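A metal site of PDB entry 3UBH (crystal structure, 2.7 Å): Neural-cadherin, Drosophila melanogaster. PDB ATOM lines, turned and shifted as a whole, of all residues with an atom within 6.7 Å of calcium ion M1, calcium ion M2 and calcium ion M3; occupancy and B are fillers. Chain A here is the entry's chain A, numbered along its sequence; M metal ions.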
ATOM      1  N   GLU A  18     -33.401  24.858 -17.870  1.00  0.00           N
ATOM      2  CA  GLU A  18     -33.201  24.811 -19.304  1.00  0.00           C
ATOM      3  C   GLU A  18     -34.175  23.872 -19.987  1.00  0.00           C
ATOM      4  O   GLU A  18     -34.921  24.279 -20.875  1.00  0.00           O
ATOM      5  CB  GLU A  18     -31.795  24.269 -19.523  1.00  0.00           C
ATOM      6  CG  GLU A  18     -31.022  24.870 -20.634  1.00  0.00           C
ATOM      7  CD  GLU A  18     -29.593  24.404 -20.607  1.00  0.00           C
ATOM      8  OE1 GLU A  18     -29.202  23.764 -19.610  1.00  0.00           O
ATOM      9  OE2 GLU A  18     -28.866  24.670 -21.582  1.00  0.00           O
ATOM     10  N   TRP A  63     -34.571  27.031 -24.907  1.00  0.00           N
ATOM     11  CA  TRP A  63     -33.832  27.634 -23.808  1.00  0.00           C
ATOM     12  C   TRP A  63     -32.462  26.982 -23.629  1.00  0.00           C
ATOM     13  O   TRP A  63     -32.297  25.768 -23.797  1.00  0.00           O
ATOM     14  CB  TRP A  63     -34.638  27.541 -22.522  1.00  0.00           C
ATOM     15  CG  TRP A  63     -35.860  28.413 -22.505  1.00  0.00           C
ATOM     16  CD1 TRP A  63     -36.338  29.208 -23.525  1.00  0.00           C
ATOM     17  CD2 TRP A  63     -36.789  28.561 -21.435  1.00  0.00           C
ATOM     18  NE1 TRP A  63     -37.491  29.843 -23.131  1.00  0.00           N
ATOM     19  CE2 TRP A  63     -37.782  29.462 -21.855  1.00  0.00           C
ATOM     20  CE3 TRP A  63     -36.863  28.015 -20.137  1.00  0.00           C
ATOM     21  CZ2 TRP A  63     -38.842  29.841 -21.040  1.00  0.00           C
ATOM     22  CZ3 TRP A  63     -37.923  28.394 -19.323  1.00  0.00           C
ATOM     23  CH2 TRP A  63     -38.910  29.288 -19.786  1.00  0.00           C
ATOM     24  N   ASP A  64     -31.484  27.814 -23.321  1.00  0.00           N
ATOM     25  CA  ASP A  64     -30.110  27.353 -23.311  1.00  0.00           C
ATOM     26  C   ASP A  64     -29.304  28.102 -22.267  1.00  0.00           C
ATOM     27  O   ASP A  64     -29.001  29.282 -22.438  1.00  0.00           O
ATOM     28  CB  ASP A  64     -29.503  27.553 -24.692  1.00  0.00           C
ATOM     29  CG  ASP A  64     -28.310  26.660 -24.929  1.00  0.00           C
ATOM     30  OD1 ASP A  64     -27.681  26.189 -23.959  1.00  0.00           O
ATOM     31  OD2 ASP A  64     -28.012  26.420 -26.115  1.00  0.00           O
ATOM     32  N   TYR A  65     -28.973  27.407 -21.190  1.00  0.00           N
ATOM     33  CA  TYR A  65     -28.137  27.937 -20.132  1.00  0.00           C
ATOM     34  C   TYR A  65     -26.791  28.347 -20.678  1.00  0.00           C
ATOM     35  O   TYR A  65     -26.261  29.384 -20.308  1.00  0.00           O
ATOM     36  CB  TYR A  65     -27.966  26.895 -19.026  1.00  0.00           C
ATOM     37  CG  TYR A  65     -27.248  27.383 -17.779  1.00  0.00           C
ATOM     38  CD1 TYR A  65     -27.955  27.996 -16.751  1.00  0.00           C
ATOM     39  CD2 TYR A  65     -25.877  27.208 -17.626  1.00  0.00           C
ATOM     40  CE1 TYR A  65     -27.317  28.440 -15.595  1.00  0.00           C
ATOM     41  CE2 TYR A  65     -25.212  27.653 -16.475  1.00  0.00           C
ATOM     42  CZ  TYR A  65     -25.950  28.271 -15.458  1.00  0.00           C
ATOM     43  OH  TYR A  65     -25.323  28.710 -14.320  1.00  0.00           O
ATOM     44  N   GLU A  66     -26.242  27.538 -21.581  1.00  0.00           N
ATOM     45  CA  GLU A  66     -24.925  27.777 -22.182  1.00  0.00           C
ATOM     46  C   GLU A  66     -24.853  29.046 -23.052  1.00  0.00           C
ATOM     47  O   GLU A  66     -23.775  29.488 -23.409  1.00  0.00           O
ATOM     48  CB  GLU A  66     -24.494  26.557 -23.009  1.00  0.00           C
ATOM     49  CG  GLU A  66     -24.027  25.354 -22.208  1.00  0.00           C
ATOM     50  CD  GLU A  66     -25.123  24.709 -21.350  1.00  0.00           C
ATOM     51  OE1 GLU A  66     -26.192  24.327 -21.868  1.00  0.00           O
ATOM     52  OE2 GLU A  66     -24.892  24.572 -20.132  1.00  0.00           O
ATOM     53  N   GLU A  67     -26.005  29.627 -23.388  1.00  0.00           N
ATOM     54  CA  GLU A  67     -26.022  30.767 -24.306  1.00  0.00           C
ATOM     55  C   GLU A  67     -26.557  32.052 -23.658  1.00  0.00           C
ATOM     56  O   GLU A  67     -26.582  33.102 -24.280  1.00  0.00           O
ATOM     57  CB  GLU A  67     -26.790  30.429 -25.580  1.00  0.00           C
ATOM     58  CG  GLU A  67     -26.047  30.787 -26.879  1.00  0.00           C
ATOM     59  CD  GLU A  67     -26.894  31.607 -27.856  1.00  0.00           C
ATOM     60  OE1 GLU A  67     -28.130  31.395 -27.929  1.00  0.00           O
ATOM     61  OE2 GLU A  67     -26.299  32.478 -28.548  1.00  0.00           O
ATOM     62  N   LYS A 102     -32.099  27.456 -14.706  1.00  0.00           N
ATOM     63  CA  LYS A 102     -31.123  26.556 -14.082  1.00  0.00           C
ATOM     64  C   LYS A 102     -30.440  25.616 -15.078  1.00  0.00           C
ATOM     65  O   LYS A 102     -31.054  25.154 -16.049  1.00  0.00           O
ATOM     66  CB  LYS A 102     -31.758  25.801 -12.908  1.00  0.00           C
ATOM     67  CG  LYS A 102     -32.025  26.695 -11.687  1.00  0.00           C
ATOM     68  CD  LYS A 102     -30.745  26.998 -10.903  1.00  0.00           C
ATOM     69  CE  LYS A 102     -30.738  28.440 -10.381  1.00  0.00           C
ATOM     70  NZ  LYS A 102     -29.753  28.654  -9.255  1.00  0.00           N
ATOM     71  N   ASP A 103     -29.168  25.353 -14.832  1.00  0.00           N
ATOM     72  CA  ASP A 103     -28.366  24.503 -15.713  1.00  0.00           C
ATOM     73  C   ASP A 103     -28.815  23.049 -15.703  1.00  0.00           C
ATOM     74  O   ASP A 103     -29.212  22.507 -14.678  1.00  0.00           O
ATOM     75  CB  ASP A 103     -26.874  24.591 -15.341  1.00  0.00           C
ATOM     76  CG  ASP A 103     -25.959  24.038 -16.428  1.00  0.00           C
ATOM     77  OD1 ASP A 103     -26.359  23.979 -17.615  1.00  0.00           O
ATOM     78  OD2 ASP A 103     -24.820  23.654 -16.095  1.00  0.00           O
ATOM     79  N   VAL A 104     -28.774  22.443 -16.879  1.00  0.00           N
ATOM     80  CA  VAL A 104     -28.930  21.009 -17.023  1.00  0.00           C
ATOM     81  C   VAL A 104     -27.757  20.545 -17.874  1.00  0.00           C
ATOM     82  O   VAL A 104     -27.395  21.198 -18.857  1.00  0.00           O
ATOM     83  CB  VAL A 104     -30.281  20.620 -17.718  1.00  0.00           C
ATOM     84  CG1 VAL A 104     -30.390  19.109 -17.906  1.00  0.00           C
ATOM     85  CG2 VAL A 104     -31.463  21.134 -16.933  1.00  0.00           C
ATOM     86  N   ASN A 105     -27.160  19.418 -17.487  1.00  0.00           N
ATOM     87  CA  ASN A 105     -26.134  18.776 -18.297  1.00  0.00           C
ATOM     88  C   ASN A 105     -26.725  18.247 -19.610  1.00  0.00           C
ATOM     89  O   ASN A 105     -27.090  17.071 -19.706  1.00  0.00           O
ATOM     90  CB  ASN A 105     -25.478  17.664 -17.499  1.00  0.00           C
ATOM     91  CG  ASN A 105     -24.209  17.173 -18.134  1.00  0.00           C
ATOM     92  OD1 ASN A 105     -24.096  17.100 -19.359  1.00  0.00           O
ATOM     93  ND2 ASN A 105     -23.226  16.816 -17.304  1.00  0.00           N
ATOM     94  N   ASP A 106     -26.787  19.102 -20.628  1.00  0.00           N
ATOM     95  CA  ASP A 106     -27.560  18.800 -21.841  1.00  0.00           C
ATOM     96  C   ASP A 106     -26.748  18.883 -23.132  1.00  0.00           C
ATOM     97  O   ASP A 106     -27.289  18.689 -24.235  1.00  0.00           O
ATOM     98  CB  ASP A 106     -28.765  19.745 -21.931  1.00  0.00           C
ATOM     99  CG  ASP A 106     -28.380  21.204 -22.149  1.00  0.00           C
ATOM    100  OD1 ASP A 106     -27.370  21.683 -21.576  1.00  0.00           O
ATOM    101  OD2 ASP A 106     -29.093  21.893 -22.898  1.00  0.00           O
ATOM    102  N   GLU A 107     -25.445  19.180 -22.993  1.00  0.00           N
ATOM    103  CA  GLU A 107     -24.556  19.303 -24.143  1.00  0.00           C
ATOM    104  C   GLU A 107     -23.448  18.273 -24.054  1.00  0.00           C
ATOM    105  O   GLU A 107     -22.829  18.109 -23.001  1.00  0.00           O
ATOM    106  CB  GLU A 107     -23.946  20.704 -24.193  1.00  0.00           C
ATOM    107  CG  GLU A 107     -24.923  21.858 -23.988  1.00  0.00           C
ATOM    108  CD  GLU A 107     -26.002  21.971 -25.043  1.00  0.00           C
ATOM    109  OE1 GLU A 107     -25.826  21.472 -26.164  1.00  0.00           O
ATOM    110  OE2 GLU A 107     -27.049  22.578 -24.743  1.00  0.00           O
ATOM    111  N   PRO A 108     -23.186  17.558 -25.173  1.00  0.00           N
ATOM    112  CA  PRO A 108     -22.177  16.484 -25.196  1.00  0.00           C
ATOM    113  C   PRO A 108     -20.755  17.033 -25.174  1.00  0.00           C
ATOM    114  O   PRO A 108     -20.547  18.178 -25.582  1.00  0.00           O
ATOM    115  CB  PRO A 108     -22.420  15.813 -26.546  1.00  0.00           C
ATOM    116  CG  PRO A 108     -22.989  16.911 -27.421  1.00  0.00           C
ATOM    117  CD  PRO A 108     -23.824  17.751 -26.492  1.00  0.00           C
ATOM    118  N   PRO A 109     -19.789  16.215 -24.718  1.00  0.00           N
ATOM    119  CA  PRO A 109     -18.392  16.585 -24.735  1.00  0.00           C
ATOM    120  C   PRO A 109     -17.835  16.497 -26.164  1.00  0.00           C
ATOM    121  O   PRO A 109     -18.484  15.899 -27.031  1.00  0.00           O
ATOM    122  CB  PRO A 109     -17.758  15.512 -23.851  1.00  0.00           C
ATOM    123  CG  PRO A 109     -18.576  14.344 -24.045  1.00  0.00           C
ATOM    124  CD  PRO A 109     -19.967  14.869 -24.152  1.00  0.00           C
ATOM    125  N   ASP A 139     -16.375  20.175 -22.347  1.00  0.00           N
ATOM    126  CA  ASP A 139     -17.815  20.013 -22.192  1.00  0.00           C
ATOM    127  C   ASP A 139     -18.429  21.317 -21.710  1.00  0.00           C
ATOM    128  O   ASP A 139     -18.023  21.850 -20.668  1.00  0.00           O
ATOM    129  CB  ASP A 139     -18.136  18.870 -21.230  1.00  0.00           C
ATOM    130  CG  ASP A 139     -19.632  18.565 -21.143  1.00  0.00           C
ATOM    131  OD1 ASP A 139     -20.392  19.395 -20.601  1.00  0.00           O
ATOM    132  OD2 ASP A 139     -20.052  17.495 -21.630  1.00  0.00           O
ATOM    133  N   PRO A 140     -19.418  21.829 -22.446  1.00  0.00           N
ATOM    134  CA  PRO A 140     -19.992  23.134 -22.198  1.00  0.00           C
ATOM    135  C   PRO A 140     -20.691  23.274 -20.849  1.00  0.00           C
ATOM    136  O   PRO A 140     -20.840  24.398 -20.377  1.00  0.00           O
ATOM    137  CB  PRO A 140     -21.011  23.297 -23.341  1.00  0.00           C
ATOM    138  CG  PRO A 140     -20.595  22.351 -24.375  1.00  0.00           C
ATOM    139  CD  PRO A 140     -20.044  21.184 -23.609  1.00  0.00           C
ATOM    140  N   ASP A 141     -21.139  22.162 -20.256  1.00  0.00           N
ATOM    141  CA  ASP A 141     -21.934  22.189 -19.024  1.00  0.00           C
ATOM    142  C   ASP A 141     -21.090  22.475 -17.789  1.00  0.00           C
ATOM    143  O   ASP A 141     -19.930  22.099 -17.739  1.00  0.00           O
ATOM    144  CB  ASP A 141     -22.688  20.870 -18.835  1.00  0.00           C
ATOM    145  CG  ASP A 141     -23.794  20.677 -19.835  1.00  0.00           C
ATOM    146  OD1 ASP A 141     -23.696  19.736 -20.654  1.00  0.00           O
ATOM    147  OD2 ASP A 141     -24.765  21.457 -19.825  1.00  0.00           O
ATOM    148  N   THR A 142     -21.691  23.119 -16.798  1.00  0.00           N
ATOM    149  CA  THR A 142     -20.975  23.581 -15.606  1.00  0.00           C
ATOM    150  C   THR A 142     -20.350  22.454 -14.782  1.00  0.00           C
ATOM    151  O   THR A 142     -19.182  22.535 -14.377  1.00  0.00           O
ATOM    152  CB  THR A 142     -21.888  24.442 -14.701  1.00  0.00           C
ATOM    153  OG1 THR A 142     -23.089  23.713 -14.395  1.00  0.00           O
ATOM    154  CG2 THR A 142     -22.254  25.764 -15.392  1.00  0.00           C
ATOM    155  N   ASP A 143     -21.126  21.387 -14.557  1.00  0.00           N
ATOM    156  CA  ASP A 143     -20.714  20.265 -13.714  1.00  0.00           C
ATOM    157  C   ASP A 143     -20.247  19.014 -14.480  1.00  0.00           C
ATOM    158  O   ASP A 143     -20.437  17.901 -14.011  1.00  0.00           O
ATOM    159  CB  ASP A 143     -21.858  19.895 -12.760  1.00  0.00           C
ATOM    160  CG  ASP A 143     -23.013  19.139 -13.458  1.00  0.00           C
ATOM    161  OD1 ASP A 143     -23.607  18.254 -12.805  1.00  0.00           O
ATOM    162  OD2 ASP A 143     -23.341  19.436 -14.642  1.00  0.00           O
ATOM    163  N   HIS A 144     -19.610  19.201 -15.643  1.00  0.00           N
ATOM    164  CA  HIS A 144     -19.131  18.075 -16.454  1.00  0.00           C
ATOM    165  C   HIS A 144     -18.182  17.104 -15.732  1.00  0.00           C
ATOM    166  O   HIS A 144     -17.567  17.441 -14.719  1.00  0.00           O
ATOM    167  CB  HIS A 144     -18.472  18.572 -17.732  1.00  0.00           C
ATOM    168  CG  HIS A 144     -17.256  19.414 -17.492  1.00  0.00           C
ATOM    169  ND1 HIS A 144     -16.054  18.887 -17.067  1.00  0.00           N
ATOM    170  CD2 HIS A 144     -17.052  20.744 -17.647  1.00  0.00           C
ATOM    171  CE1 HIS A 144     -15.168  19.867 -16.956  1.00  0.00           C
ATOM    172  NE2 HIS A 144     -15.749  20.998 -17.301  1.00  0.00           N
ATOM    173  N   ASN A 145     -18.074  15.899 -16.255  1.00  0.00           N
ATOM    174  CA  ASN A 145     -17.281  14.868 -15.614  1.00  0.00           C
ATOM    175  C   ASN A 145     -16.711  13.968 -16.689  1.00  0.00           C
ATOM    176  O   ASN A 145     -17.262  12.908 -16.994  1.00  0.00           O
ATOM    177  CB  ASN A 145     -18.129  14.080 -14.611  1.00  0.00           C
ATOM    178  CG  ASN A 145     -17.322  13.079 -13.812  1.00  0.00           C
ATOM    179  OD1 ASN A 145     -16.093  12.980 -13.948  1.00  0.00           O
ATOM    180  ND2 ASN A 145     -18.008  12.315 -12.970  1.00  0.00           N
ATOM    181  N   ASP A 190     -19.202  12.242 -20.724  1.00  0.00           N
ATOM    182  CA  ASP A 190     -19.510  13.081 -19.580  1.00  0.00           C
ATOM    183  C   ASP A 190     -20.480  12.296 -18.715  1.00  0.00           C
ATOM    184  O   ASP A 190     -21.633  12.086 -19.089  1.00  0.00           O
ATOM    185  CB  ASP A 190     -20.115  14.411 -20.059  1.00  0.00           C
ATOM    186  CG  ASP A 190     -20.570  15.289 -18.916  1.00  0.00           C
ATOM    187  OD1 ASP A 190     -20.233  15.017 -17.749  1.00  0.00           O
ATOM    188  OD2 ASP A 190     -21.270  16.284 -19.216  1.00  0.00           O
ATOM    189  N   ASN A 192     -21.743  12.973 -15.826  1.00  0.00           N
ATOM    190  CA  ASN A 192     -22.733  13.726 -15.091  1.00  0.00           C
ATOM    191  C   ASN A 192     -23.979  13.972 -15.928  1.00  0.00           C
ATOM    192  O   ASN A 192     -24.989  14.449 -15.410  1.00  0.00           O
ATOM    193  CB  ASN A 192     -22.135  15.022 -14.548  1.00  0.00           C
ATOM    194  CG  ASN A 192     -21.403  14.821 -13.228  1.00  0.00           C
ATOM    195  OD1 ASN A 192     -21.061  13.705 -12.842  1.00  0.00           O
ATOM    196  ND2 ASN A 192     -21.150  15.915 -12.526  1.00  0.00           N
ATOM    197  N   GLY A 193     -23.911  13.630 -17.214  1.00  0.00           N
ATOM    198  CA  GLY A 193     -25.074  13.717 -18.120  1.00  0.00           C
ATOM    199  C   GLY A 193     -25.366  12.449 -18.932  1.00  0.00           C
ATOM    200  O   GLY A 193     -24.445  11.766 -19.378  1.00  0.00           O
ATOM    201  N   GLN A 201     -23.693  10.784 -22.172  1.00  0.00           N
ATOM    202  CA  GLN A 201     -23.290  11.722 -23.222  1.00  0.00           C
ATOM    203  C   GLN A 201     -21.882  11.364 -23.664  1.00  0.00           C
ATOM    204  O   GLN A 201     -21.063  10.947 -22.841  1.00  0.00           O
ATOM    205  CB  GLN A 201     -23.245  13.148 -22.696  1.00  0.00           C
ATOM    206  CG  GLN A 201     -24.575  13.834 -22.484  1.00  0.00           C
ATOM    207  CD  GLN A 201     -24.372  15.195 -21.836  1.00  0.00           C
ATOM    208  OE1 GLN A 201     -23.229  15.638 -21.655  1.00  0.00           O
ATOM    209  NE2 GLN A 201     -25.453  15.848 -21.477  1.00  0.00           N
HETATM  210 CA    CA M   1     -28.098  24.050 -23.391  1.00  0.00          CA
HETATM  211 CA    CA M   2     -26.506  22.944 -19.682  1.00  0.00          CA
HETATM  212 CA    CA M   3     -22.187  17.656 -20.767  1.00  0.00          CA
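Within 4 Å of calcium ion M1: Glu 18, Asp 64, Glu 66, Asp 106 and Glu 107.
The nearest printed residue that does not touch calcium ion M1 is Tyr 65 (4.1 Å).
Calcium ion M3 is bound by OD2 of Asp 190 (2.3 Å), OD2 of Asp 139 (2.3 Å), O of Glu 107 (2.4 Å), OD1 of Asn 105 (2.4 Å), OE1 of Gln 201 (2.4 Å), OD1 of Asp 139 (2.5 Å) and OD1 of Asp 141 (2.6 Å).
Calcium ion M3 has seven donor atoms within binding distance.
Calcium ion M2 is bound by O of Val 104.
The side-chain carboxylate (OD2) of Asp 141 binds calcium ion M2 (2.3 Å).
Calcium ion M2 is bound by OD1 of Asp 103 (2.3 Å).
Calcium ion M2 is bound by OE2 of Glu 66 (2.3 Å).
OD1 of Asp 106 is bound to calcium ion M2 (2.4 Å).
Calcium ion M2 is bound by the side-chain carboxylate (OE1) of Glu 66, at 2.6 Å.
OE1 of Glu 18 binds calcium ion M2, at 2.8 Å.
Calcium ion M2 has seven donor atoms within binding distance.
Six residues have an atom within 4 Å of calcium ion M2: Glu 18, Glu 66, Asp 103, Val 104, Asp 106 and Asp 141.
Of the 25 residues printed, 6 come within 4 Å of calcium ion M3.
The nearest printed residue that does not touch calcium ion M3 is Pro 108 (4.5 Å).
N of Tyr 65 sits close to OE2 of Glu 18, at 2.8 Å.
The backbone NH (N) of Glu 18 sits at hydrogen-bond distance from the backbone carbonyl oxygen (O) of Lys 102 (3.0 Å).
OD1 of Asp 190 lies within hydrogen-bond range of N of Asn 192 (3.2 Å).
The backbone NH (N) of Asn 145 lies within hydrogen-bond range of the side-chain carboxylate (OD1) of Asp 190, at 2.8 Å.
OD2 of Asp 103 is in hydrogen-bond range of OG1 of Thr 142 (2.4 Å).
ND2 of Asn 105 sits close to N of Gly 193 (3.3 Å).
The backbone NH (N) of Gln 201 lies within hydrogen-bond range of the backbone carbonyl oxygen (O) of Gly 193 (3.1 Å).
Calcium ion M1 is bound by OE2 of Glu 18 (2.1 Å), OD1 of Asp 64 (2.3 Å), OE2 of Glu 107 (2.3 Å), OD2 of Asp 106 (2.4 Å) and OE1 of Glu 66 (2.5 Å).
Slightly farther from calcium ion M1 lies OD1 of Asp 106 (3.1 Å).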
